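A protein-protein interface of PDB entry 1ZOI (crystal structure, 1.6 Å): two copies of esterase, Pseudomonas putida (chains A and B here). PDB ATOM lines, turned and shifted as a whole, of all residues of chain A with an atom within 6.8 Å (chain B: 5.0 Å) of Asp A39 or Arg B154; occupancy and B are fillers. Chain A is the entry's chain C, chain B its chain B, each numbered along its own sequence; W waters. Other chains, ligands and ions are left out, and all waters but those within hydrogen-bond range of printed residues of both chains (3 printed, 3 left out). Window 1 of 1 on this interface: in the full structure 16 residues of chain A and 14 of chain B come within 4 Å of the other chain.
The side-chain carboxylate (OD2) of Asp A39 lies within salt-bridge range of the guanidinium group (NH2) of Arg B154, 3.1 Å away. N of Gly A179 sits at hydrogen-bond distance from OE1 of Gln B156, 3.0 Å away.
The backbone carbonyl oxygen of Gln B149 is in hydrogen-bond range of the backbone NH of Arg B154, 3.2 Å away. The backbone carbonyl oxygen of Gly B188 lies within hydrogen-bond range of the guanidinium group of Arg B154. The guanidinium group (NH1) of Arg B154 is in hydrogen-bond range of the backbone carbonyl oxygen (O) of Gly B191, at 3.0 Å. The guanidinium group (NH1) of Arg B154 lies within hydrogen-bond range of a ring nitrogen (ND1) of His B196, 3.1 Å away. The side-chain amino group (NZ) of Lys A15 lies within salt-bridge range of the side-chain carboxylate (OD1) of Asp A36. The guanidinium group (NH2) of Arg A186 is in salt-bridge range of the side-chain carboxylate (OD2) of Asp A36, 2.9 Å away.
Among the printed residues, pairs that only touch across the chains: Trp A17 with Ser B192 (3.3 Å), Gly A179 with Ala B155 (3.4 Å), Ala A40 with Ala B151 (3.4 Å), Asn A183 with Met B189 (3.4 Å), Leu A43 with Ala B151 (3.5 Å), Arg A186 with Met B189 (3.7 Å), Asp A36 with Met B189 (3.7 Å), Leu A43 with Val B150 (3.9 Å), Arg A186 with Ile B190 (3.9 Å), Leu A43 with Ala B193 (3.9 Å) and Asp A39 with Ala B193 (3.96 Å).
Asp A39 touches just these residues of chain B: Arg B154 and Ala B193. Of the printed residues of chain B, Gly A179 touches Ala B155 and Gln B156. Of the printed residues of chain B, Arg A186 touches Met B189 and Ile B190. Arg B154 touches one residue of chain A. Of the printed residues of chain A, Ala B155 touches Gly A179.
Among the printed residues, 13 pairs touch across the chains. Among the printed residues, Asp or Glu carboxylates within 4 Å of a Lys or Arg side-chain nitrogen of the other chain: Asp A39 with Arg B154.
No position is printed for both chains.
Water W2 lies within hydrogen-bond range of the side-chain hydroxyl of Ser B192 and the indole nitrogen of Trp A17. Water W3 bridges the backbone carbonyl oxygen of Ala A40 (2.7 Å) and the backbone carbonyl oxygen of Ala B151 (2.8 Å). Water W1 lies within hydrogen-bond range of the side-chain carboxylate of Asp A39, the backbone carbonyl oxygen of Asp A36, the side-chain amide nitrogen of Asn A183 and the guanidinium group of Arg B154.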
ATOM      1  N   LYS A  15     -25.701  -0.510 -11.860  1.00  0.00           N
ATOM      2  CA  LYS A  15     -24.459  -0.982 -11.273  1.00  0.00           C
ATOM      3  C   LYS A  15     -23.769  -1.696 -12.417  1.00  0.00           C
ATOM      4  O   LYS A  15     -24.418  -2.374 -13.217  1.00  0.00           O
ATOM      5  CB  LYS A  15     -24.730  -1.970 -10.140  1.00  0.00           C
ATOM      6  CG  LYS A  15     -25.575  -1.408  -9.015  1.00  0.00           C
ATOM      7  CD  LYS A  15     -25.624  -2.378  -7.861  1.00  0.00           C
ATOM      8  CE  LYS A  15     -26.378  -1.781  -6.683  1.00  0.00           C
ATOM      9  NZ  LYS A  15     -26.092  -2.528  -5.422  1.00  0.00           N
ATOM     10  N   TRP A  17     -20.172  -3.819 -12.595  1.00  0.00           N
ATOM     11  CA  TRP A  17     -18.963  -4.290 -11.927  1.00  0.00           C
ATOM     12  C   TRP A  17     -18.193  -5.318 -12.746  1.00  0.00           C
ATOM     13  O   TRP A  17     -18.785  -6.114 -13.474  1.00  0.00           O
ATOM     14  CB  TRP A  17     -19.312  -4.911 -10.566  1.00  0.00           C
ATOM     15  CG  TRP A  17     -20.082  -4.015  -9.624  1.00  0.00           C
ATOM     16  CD1 TRP A  17     -20.116  -2.648  -9.630  1.00  0.00           C
ATOM     17  CD2 TRP A  17     -20.877  -4.430  -8.502  1.00  0.00           C
ATOM     18  NE1 TRP A  17     -20.881  -2.188  -8.582  1.00  0.00           N
ATOM     19  CE2 TRP A  17     -21.359  -3.259  -7.873  1.00  0.00           C
ATOM     20  CE3 TRP A  17     -21.227  -5.680  -7.965  1.00  0.00           C
ATOM     21  CZ2 TRP A  17     -22.174  -3.297  -6.732  1.00  0.00           C
ATOM     22  CZ3 TRP A  17     -22.038  -5.718  -6.828  1.00  0.00           C
ATOM     23  CH2 TRP A  17     -22.501  -4.528  -6.226  1.00  0.00           C
ATOM     24  N   ALA A  35     -31.932  -3.097  -8.325  1.00  0.00           N
ATOM     25  CA  ALA A  35     -30.711  -3.839  -8.623  1.00  0.00           C
ATOM     26  C   ALA A  35     -30.063  -4.398  -7.351  1.00  0.00           C
ATOM     27  O   ALA A  35     -29.256  -5.325  -7.415  1.00  0.00           O
ATOM     28  CB  ALA A  35     -29.722  -2.944  -9.361  1.00  0.00           C
ATOM     29  N   ASP A  36     -30.415  -3.839  -6.194  1.00  0.00           N
ATOM     30  CA  ASP A  36     -29.861  -4.319  -4.928  1.00  0.00           C
ATOM     31  C   ASP A  36     -30.329  -5.734  -4.600  1.00  0.00           C
ATOM     32  O   ASP A  36     -29.750  -6.407  -3.742  1.00  0.00           O
ATOM     33  CB  ASP A  36     -30.265  -3.392  -3.780  1.00  0.00           C
ATOM     34  CG  ASP A  36     -29.394  -2.157  -3.693  1.00  0.00           C
ATOM     35  OD1 ASP A  36     -28.642  -1.889  -4.649  1.00  0.00           O
ATOM     36  OD2 ASP A  36     -29.475  -1.450  -2.664  1.00  0.00           O
ATOM     37  N   ASP A  37     -31.373  -6.190  -5.281  1.00  0.00           N
ATOM     38  CA  ASP A  37     -31.902  -7.522  -5.014  1.00  0.00           C
ATOM     39  C   ASP A  37     -31.017  -8.631  -5.579  1.00  0.00           C
ATOM     40  O   ASP A  37     -31.265  -9.810  -5.335  1.00  0.00           O
ATOM     41  CB  ASP A  37     -33.312  -7.653  -5.599  1.00  0.00           C
ATOM     42  CG  ASP A  37     -34.097  -8.786  -4.969  1.00  0.00           C
ATOM     43  OD1 ASP A  37     -34.204  -8.794  -3.728  1.00  0.00           O
ATOM     44  OD2 ASP A  37     -34.606  -9.658  -5.707  1.00  0.00           O
ATOM     45  N   TRP A  38     -29.982  -8.250  -6.323  1.00  0.00           N
ATOM     46  CA  TRP A  38     -29.096  -9.229  -6.949  1.00  0.00           C
ATOM     47  C   TRP A  38     -27.738  -9.450  -6.283  1.00  0.00           C
ATOM     48  O   TRP A  38     -26.900 -10.144  -6.849  1.00  0.00           O
ATOM     49  CB  TRP A  38     -28.840  -8.840  -8.410  1.00  0.00           C
ATOM     50  CG  TRP A  38     -30.018  -8.971  -9.322  1.00  0.00           C
ATOM     51  CD1 TRP A  38     -30.717  -7.953  -9.910  1.00  0.00           C
ATOM     52  CD2 TRP A  38     -30.616 -10.188  -9.780  1.00  0.00           C
ATOM     53  NE1 TRP A  38     -31.711  -8.466 -10.712  1.00  0.00           N
ATOM     54  CE2 TRP A  38     -31.671  -9.833 -10.651  1.00  0.00           C
ATOM     55  CE3 TRP A  38     -30.363 -11.548  -9.541  1.00  0.00           C
ATOM     56  CZ2 TRP A  38     -32.472 -10.788 -11.287  1.00  0.00           C
ATOM     57  CZ3 TRP A  38     -31.161 -12.497 -10.173  1.00  0.00           C
ATOM     58  CH2 TRP A  38     -32.204 -12.110 -11.037  1.00  0.00           C
ATOM     59  N   ASP A  39     -27.514  -8.881  -5.098  1.00  0.00           N
ATOM     60  CA  ASP A  39     -26.221  -9.024  -4.420  1.00  0.00           C
ATOM     61  C   ASP A  39     -25.514 -10.376  -4.569  1.00  0.00           C
ATOM     62  O   ASP A  39     -24.380 -10.447  -5.053  1.00  0.00           O
ATOM     63  CB  ASP A  39     -26.360  -8.733  -2.921  1.00  0.00           C
ATOM     64  CG  ASP A  39     -26.505  -7.253  -2.605  1.00  0.00           C
ATOM     65  OD1 ASP A  39     -26.293  -6.401  -3.494  1.00  0.00           O
ATOM     66  OD2 ASP A  39     -26.826  -6.946  -1.437  1.00  0.00           O
ATOM     67  N   ALA A  40     -26.176 -11.445  -4.136  1.00  0.00           N
ATOM     68  CA  ALA A  40     -25.581 -12.775  -4.199  1.00  0.00           C
ATOM     69  C   ALA A  40     -25.164 -13.181  -5.607  1.00  0.00           C
ATOM     70  O   ALA A  40     -24.102 -13.770  -5.794  1.00  0.00           O
ATOM     71  CB  ALA A  40     -26.539 -13.808  -3.619  1.00  0.00           C
ATOM     72  N   GLN A  41     -25.993 -12.871  -6.598  1.00  0.00           N
ATOM     73  CA  GLN A  41     -25.656 -13.215  -7.977  1.00  0.00           C
ATOM     74  C   GLN A  41     -24.527 -12.349  -8.524  1.00  0.00           C
ATOM     75  O   GLN A  41     -23.641 -12.839  -9.223  1.00  0.00           O
ATOM     76  CB  GLN A  41     -26.881 -13.075  -8.885  1.00  0.00           C
ATOM     77  CG  GLN A  41     -27.862 -14.229  -8.807  1.00  0.00           C
ATOM     78  CD  GLN A  41     -28.546 -14.334  -7.460  1.00  0.00           C
ATOM     79  OE1 GLN A  41     -29.117 -13.363  -6.967  1.00  0.00           O
ATOM     80  NE2 GLN A  41     -28.505 -15.524  -6.863  1.00  0.00           N
ATOM     81  N   LEU A  42     -24.551 -11.055  -8.219  1.00  0.00           N
ATOM     82  CA  LEU A  42     -23.504 -10.184  -8.732  1.00  0.00           C
ATOM     83  C   LEU A  42     -22.132 -10.624  -8.234  1.00  0.00           C
ATOM     84  O   LEU A  42     -21.190 -10.730  -9.020  1.00  0.00           O
ATOM     85  CB  LEU A  42     -23.770  -8.725  -8.337  1.00  0.00           C
ATOM     86  CG  LEU A  42     -25.086  -8.122  -8.837  1.00  0.00           C
ATOM     87  CD1 LEU A  42     -25.099  -6.639  -8.501  1.00  0.00           C
ATOM     88  CD2 LEU A  42     -25.231  -8.316 -10.345  1.00  0.00           C
ATOM     89  N   LEU A  43     -22.015 -10.891  -6.935  1.00  0.00           N
ATOM     90  CA  LEU A  43     -20.725 -11.303  -6.394  1.00  0.00           C
ATOM     91  C   LEU A  43     -20.292 -12.670  -6.905  1.00  0.00           C
ATOM     92  O   LEU A  43     -19.107 -12.895  -7.174  1.00  0.00           O
ATOM     93  CB  LEU A  43     -20.750 -11.295  -4.859  1.00  0.00           C
ATOM     94  CG  LEU A  43     -20.761  -9.904  -4.216  1.00  0.00           C
ATOM     95  CD1 LEU A  43     -20.560 -10.019  -2.718  1.00  0.00           C
ATOM     96  CD2 LEU A  43     -19.660  -9.065  -4.811  1.00  0.00           C
ATOM     97  N   PHE A  44     -21.246 -13.583  -7.046  1.00  0.00           N
ATOM     98  CA  PHE A  44     -20.929 -14.920  -7.527  1.00  0.00           C
ATOM     99  C   PHE A  44     -20.374 -14.855  -8.938  1.00  0.00           C
ATOM    100  O   PHE A  44     -19.325 -15.422  -9.231  1.00  0.00           O
ATOM    101  CB  PHE A  44     -22.180 -15.805  -7.522  1.00  0.00           C
ATOM    102  CG  PHE A  44     -21.936 -17.208  -8.019  1.00  0.00           C
ATOM    103  CD1 PHE A  44     -21.508 -18.205  -7.147  1.00  0.00           C
ATOM    104  CD2 PHE A  44     -22.123 -17.527  -9.359  1.00  0.00           C
ATOM    105  CE1 PHE A  44     -21.273 -19.504  -7.608  1.00  0.00           C
ATOM    106  CE2 PHE A  44     -21.890 -18.820  -9.829  1.00  0.00           C
ATOM    107  CZ  PHE A  44     -21.465 -19.809  -8.949  1.00  0.00           C
ATOM    108  N   GLY A 179     -33.563  -9.522   8.203  1.00  0.00           N
ATOM    109  CA  GLY A 179     -32.698  -8.766   7.311  1.00  0.00           C
ATOM    110  C   GLY A 179     -33.191  -8.848   5.880  1.00  0.00           C
ATOM    111  O   GLY A 179     -33.264  -7.840   5.169  1.00  0.00           O
ATOM    112  N   ASN A 183     -34.789  -5.798   3.768  1.00  0.00           N
ATOM    113  CA  ASN A 183     -34.158  -5.339   2.536  1.00  0.00           C
ATOM    114  C   ASN A 183     -35.167  -5.283   1.390  1.00  0.00           C
ATOM    115  O   ASN A 183     -35.094  -4.406   0.528  1.00  0.00           O
ATOM    116  CB  ASN A 183     -32.981  -6.244   2.180  1.00  0.00           C
ATOM    117  CG  ASN A 183     -32.017  -5.582   1.222  1.00  0.00           C
ATOM    118  OD1 ASN A 183     -31.764  -4.376   1.314  1.00  0.00           O
ATOM    119  ND2 ASN A 183     -31.459  -6.365   0.308  1.00  0.00           N
ATOM    120  N   ARG A 186     -37.201  -2.239   2.172  1.00  0.00           N
ATOM    121  CA  ARG A 186     -36.372  -1.062   1.900  1.00  0.00           C
ATOM    122  C   ARG A 186     -36.334  -0.689   0.422  1.00  0.00           C
ATOM    123  O   ARG A 186     -36.514   0.475   0.062  1.00  0.00           O
ATOM    124  CB  ARG A 186     -34.942  -1.314   2.381  1.00  0.00           C
ATOM    125  CG  ARG A 186     -34.000  -0.119   2.228  1.00  0.00           C
ATOM    126  CD  ARG A 186     -32.583  -0.519   2.617  1.00  0.00           C
ATOM    127  NE  ARG A 186     -32.006  -1.499   1.700  1.00  0.00           N
ATOM    128  CZ  ARG A 186     -31.473  -1.196   0.521  1.00  0.00           C
ATOM    129  NH1 ARG A 186     -31.443   0.066   0.110  1.00  0.00           N
ATOM    130  NH2 ARG A 186     -30.956  -2.148  -0.239  1.00  0.00           N
ATOM    131  N   GLN B 149     -20.046 -14.371   4.217  1.00  0.00           N
ATOM    132  CA  GLN B 149     -21.341 -13.862   4.655  1.00  0.00           C
ATOM    133  C   GLN B 149     -21.776 -12.685   3.786  1.00  0.00           C
ATOM    134  O   GLN B 149     -22.939 -12.582   3.403  1.00  0.00           O
ATOM    135  CB  GLN B 149     -21.269 -13.418   6.115  1.00  0.00           C
ATOM    136  CG  GLN B 149     -21.300 -14.561   7.116  1.00  0.00           C
ATOM    137  CD  GLN B 149     -22.627 -15.284   7.099  1.00  0.00           C
ATOM    138  OE1 GLN B 149     -22.715 -16.442   6.677  1.00  0.00           O
ATOM    139  NE2 GLN B 149     -23.677 -14.599   7.544  1.00  0.00           N
ATOM    140  N   VAL B 150     -20.839 -11.798   3.469  1.00  0.00           N
ATOM    141  CA  VAL B 150     -21.172 -10.644   2.640  1.00  0.00           C
ATOM    142  C   VAL B 150     -21.594 -11.104   1.249  1.00  0.00           C
ATOM    143  O   VAL B 150     -22.472 -10.509   0.624  1.00  0.00           O
ATOM    144  CB  VAL B 150     -19.971  -9.681   2.501  1.00  0.00           C
ATOM    145  CG1 VAL B 150     -20.301  -8.564   1.507  1.00  0.00           C
ATOM    146  CG2 VAL B 150     -19.619  -9.090   3.856  1.00  0.00           C
ATOM    147  N   ALA B 151     -20.975 -12.176   0.772  1.00  0.00           N
ATOM    148  CA  ALA B 151     -21.278 -12.689  -0.556  1.00  0.00           C
ATOM    149  C   ALA B 151     -22.602 -13.436  -0.693  1.00  0.00           C
ATOM    150  O   ALA B 151     -23.258 -13.330  -1.726  1.00  0.00           O
ATOM    151  CB  ALA B 151     -20.134 -13.581  -1.036  1.00  0.00           C
ATOM    152  N   SER B 152     -23.010 -14.169   0.341  1.00  0.00           N
ATOM    153  CA  SER B 152     -24.236 -14.960   0.254  1.00  0.00           C
ATOM    154  C   SER B 152     -25.433 -14.624   1.148  1.00  0.00           C
ATOM    155  O   SER B 152     -26.529 -15.124   0.900  1.00  0.00           O
ATOM    156  CB  SER B 152     -23.891 -16.443   0.419  1.00  0.00           C
ATOM    157  OG  SER B 152     -23.201 -16.673   1.636  1.00  0.00           O
ATOM    158  N   ASN B 153     -25.243 -13.825   2.196  1.00  0.00           N
ATOM    159  CA  ASN B 153     -26.373 -13.450   3.047  1.00  0.00           C
ATOM    160  C   ASN B 153     -26.072 -12.141   3.753  1.00  0.00           C
ATOM    161  O   ASN B 153     -26.114 -12.036   4.982  1.00  0.00           O
ATOM    162  CB  ASN B 153     -26.712 -14.550   4.063  1.00  0.00           C
ATOM    163  CG  ASN B 153     -25.684 -14.678   5.156  1.00  0.00           C
ATOM    164  OD1 ASN B 153     -26.000 -15.106   6.267  1.00  0.00           O
ATOM    165  ND2 ASN B 153     -24.442 -14.321   4.852  1.00  0.00           N
ATOM    166  N   ARG B 154     -25.786 -11.130   2.944  1.00  0.00           N
ATOM    167  CA  ARG B 154     -25.443  -9.811   3.446  1.00  0.00           C
ATOM    168  C   ARG B 154     -26.549  -9.153   4.260  1.00  0.00           C
ATOM    169  O   ARG B 154     -26.281  -8.555   5.297  1.00  0.00           O
ATOM    170  CB  ARG B 154     -25.040  -8.898   2.276  1.00  0.00           C
ATOM    171  CG  ARG B 154     -24.311  -7.630   2.726  1.00  0.00           C
ATOM    172  CD  ARG B 154     -23.805  -6.750   1.561  1.00  0.00           C
ATOM    173  NE  ARG B 154     -24.891  -6.087   0.839  1.00  0.00           N
ATOM    174  CZ  ARG B 154     -24.920  -4.789   0.545  1.00  0.00           C
ATOM    175  NH1 ARG B 154     -23.921  -3.993   0.906  1.00  0.00           N
ATOM    176  NH2 ARG B 154     -25.956  -4.280  -0.111  1.00  0.00           N
ATOM    177  N   ALA B 155     -27.790  -9.261   3.793  1.00  0.00           N
ATOM    178  CA  ALA B 155     -28.918  -8.646   4.486  1.00  0.00           C
ATOM    179  C   ALA B 155     -29.090  -9.116   5.931  1.00  0.00           C
ATOM    180  O   ALA B 155     -29.378  -8.308   6.812  1.00  0.00           O
ATOM    181  CB  ALA B 155     -30.209  -8.873   3.703  1.00  0.00           C
ATOM    182  N   GLN B 156     -28.926 -10.413   6.185  1.00  0.00           N
ATOM    183  CA  GLN B 156     -29.071 -10.902   7.554  1.00  0.00           C
ATOM    184  C   GLN B 156     -27.787 -10.692   8.348  1.00  0.00           C
ATOM    185  O   GLN B 156     -27.829 -10.365   9.531  1.00  0.00           O
ATOM    186  CB  GLN B 156     -29.447 -12.383   7.578  1.00  0.00           C
ATOM    187  CG  GLN B 156     -29.733 -12.899   8.986  1.00  0.00           C
ATOM    188  CD  GLN B 156     -30.796 -12.084   9.701  1.00  0.00           C
ATOM    189  OE1 GLN B 156     -31.873 -11.832   9.154  1.00  0.00           O
ATOM    190  NE2 GLN B 156     -30.502 -11.668  10.932  1.00  0.00           N
ATOM    191  N   PHE B 157     -26.647 -10.879   7.690  1.00  0.00           N
ATOM    192  CA  PHE B 157     -25.349 -10.686   8.328  1.00  0.00           C
ATOM    193  C   PHE B 157     -25.241  -9.259   8.882  1.00  0.00           C
ATOM    194  O   PHE B 157     -24.691  -9.043   9.960  1.00  0.00           O
ATOM    195  CB  PHE B 157     -24.231 -10.946   7.308  1.00  0.00           C
ATOM    196  CG  PHE B 157     -22.837 -10.807   7.865  1.00  0.00           C
ATOM    197  CD1 PHE B 157     -22.453 -11.486   9.020  1.00  0.00           C
ATOM    198  CD2 PHE B 157     -21.885 -10.029   7.204  1.00  0.00           C
ATOM    199  CE1 PHE B 157     -21.144 -11.395   9.502  1.00  0.00           C
ATOM    200  CE2 PHE B 157     -20.578  -9.930   7.674  1.00  0.00           C
ATOM    201  CZ  PHE B 157     -20.204 -10.615   8.827  1.00  0.00           C
ATOM    202  N   TYR B 158     -25.779  -8.286   8.148  1.00  0.00           N
ATOM    203  CA  TYR B 158     -25.715  -6.894   8.583  1.00  0.00           C
ATOM    204  C   TYR B 158     -26.681  -6.573   9.711  1.00  0.00           C
ATOM    205  O   TYR B 158     -26.772  -5.435  10.168  1.00  0.00           O
ATOM    206  CB  TYR B 158     -25.942  -5.952   7.399  1.00  0.00           C
ATOM    207  CG  TYR B 158     -24.732  -5.808   6.510  1.00  0.00           C
ATOM    208  CD1 TYR B 158     -24.716  -4.872   5.475  1.00  0.00           C
ATOM    209  CD2 TYR B 158     -23.599  -6.614   6.690  1.00  0.00           C
ATOM    210  CE1 TYR B 158     -23.609  -4.741   4.642  1.00  0.00           C
ATOM    211  CE2 TYR B 158     -22.491  -6.491   5.859  1.00  0.00           C
ATOM    212  CZ  TYR B 158     -22.505  -5.549   4.838  1.00  0.00           C
ATOM    213  OH  TYR B 158     -21.406  -5.405   4.019  1.00  0.00           O
ATOM    214  N   GLY B 188     -25.216  -0.104   5.848  1.00  0.00           N
ATOM    215  CA  GLY B 188     -24.553  -1.194   5.169  1.00  0.00           C
ATOM    216  C   GLY B 188     -25.257  -1.573   3.878  1.00  0.00           C
ATOM    217  O   GLY B 188     -24.609  -1.744   2.851  1.00  0.00           O
ATOM    218  N   MET B 189     -26.585  -1.683   3.910  1.00  0.00           N
ATOM    219  CA  MET B 189     -27.306  -2.100   2.714  1.00  0.00           C
ATOM    220  C   MET B 189     -27.287  -1.129   1.536  1.00  0.00           C
ATOM    221  O   MET B 189     -27.403  -1.557   0.384  1.00  0.00           O
ATOM    222  CB  MET B 189     -28.745  -2.487   3.067  1.00  0.00           C
ATOM    223  CG  MET B 189     -28.841  -3.655   4.056  1.00  0.00           C
ATOM    224  SD  MET B 189     -27.790  -5.087   3.643  1.00  0.00           S
ATOM    225  CE  MET B 189     -28.667  -5.715   2.217  1.00  0.00           C
ATOM    226  N   ILE B 190     -27.131   0.166   1.797  1.00  0.00           N
ATOM    227  CA  ILE B 190     -27.087   1.116   0.685  1.00  0.00           C
ATOM    228  C   ILE B 190     -25.715   1.116   0.012  1.00  0.00           C
ATOM    229  O   ILE B 190     -25.555   1.645  -1.090  1.00  0.00           O
ATOM    230  CB  ILE B 190     -27.456   2.553   1.129  1.00  0.00           C
ATOM    231  CG1 ILE B 190     -26.495   3.060   2.207  1.00  0.00           C
ATOM    232  CG2 ILE B 190     -28.897   2.572   1.629  1.00  0.00           C
ATOM    233  CD1 ILE B 190     -26.748   4.516   2.590  1.00  0.00           C
ATOM    234  N   GLY B 191     -24.730   0.509   0.671  1.00  0.00           N
ATOM    235  CA  GLY B 191     -23.397   0.423   0.096  1.00  0.00           C
ATOM    236  C   GLY B 191     -23.281  -0.763  -0.852  1.00  0.00           C
ATOM    237  O   GLY B 191     -24.183  -1.597  -0.933  1.00  0.00           O
ATOM    238  N   SER B 192     -22.162  -0.843  -1.563  1.00  0.00           N
ATOM    239  CA  SER B 192     -21.911  -1.919  -2.517  1.00  0.00           C
ATOM    240  C   SER B 192     -21.438  -3.211  -1.859  1.00  0.00           C
ATOM    241  O   SER B 192     -20.488  -3.205  -1.074  1.00  0.00           O
ATOM    242  CB  SER B 192     -20.848  -1.473  -3.517  1.00  0.00           C
ATOM    243  OG  SER B 192     -20.231  -2.602  -4.105  1.00  0.00           O
ATOM    244  N   ALA B 193     -22.088  -4.327  -2.187  1.00  0.00           N
ATOM    245  CA  ALA B 193     -21.680  -5.606  -1.617  1.00  0.00           C
ATOM    246  C   ALA B 193     -20.244  -5.928  -2.030  1.00  0.00           C
ATOM    247  O   ALA B 193     -19.496  -6.525  -1.262  1.00  0.00           O
ATOM    248  CB  ALA B 193     -22.614  -6.720  -2.077  1.00  0.00           C
ATOM    249  N   HIS B 196     -17.850  -3.788   0.023  1.00  0.00           N
ATOM    250  CA  HIS B 196     -17.765  -4.321   1.377  1.00  0.00           C
ATOM    251  C   HIS B 196     -16.984  -5.631   1.407  1.00  0.00           C
ATOM    252  O   HIS B 196     -16.209  -5.877   2.333  1.00  0.00           O
ATOM    253  CB  HIS B 196     -19.168  -4.523   1.940  1.00  0.00           C
ATOM    254  CG  HIS B 196     -19.907  -3.243   2.163  1.00  0.00           C
ATOM    255  ND1 HIS B 196     -21.266  -3.199   2.385  1.00  0.00           N
ATOM    256  CD2 HIS B 196     -19.477  -1.958   2.198  1.00  0.00           C
ATOM    257  CE1 HIS B 196     -21.645  -1.944   2.542  1.00  0.00           C
ATOM    258  NE2 HIS B 196     -20.579  -1.170   2.433  1.00  0.00           N
HETATM  259  O   HOH W   1     -29.076  -5.297  -1.134  1.00  0.00           O
HETATM  260  O   HOH W   2     -18.864  -1.896  -6.277  1.00  0.00           O
HETATM  261  O   HOH W   3     -22.671 -15.014  -3.838  1.00  0.00           O
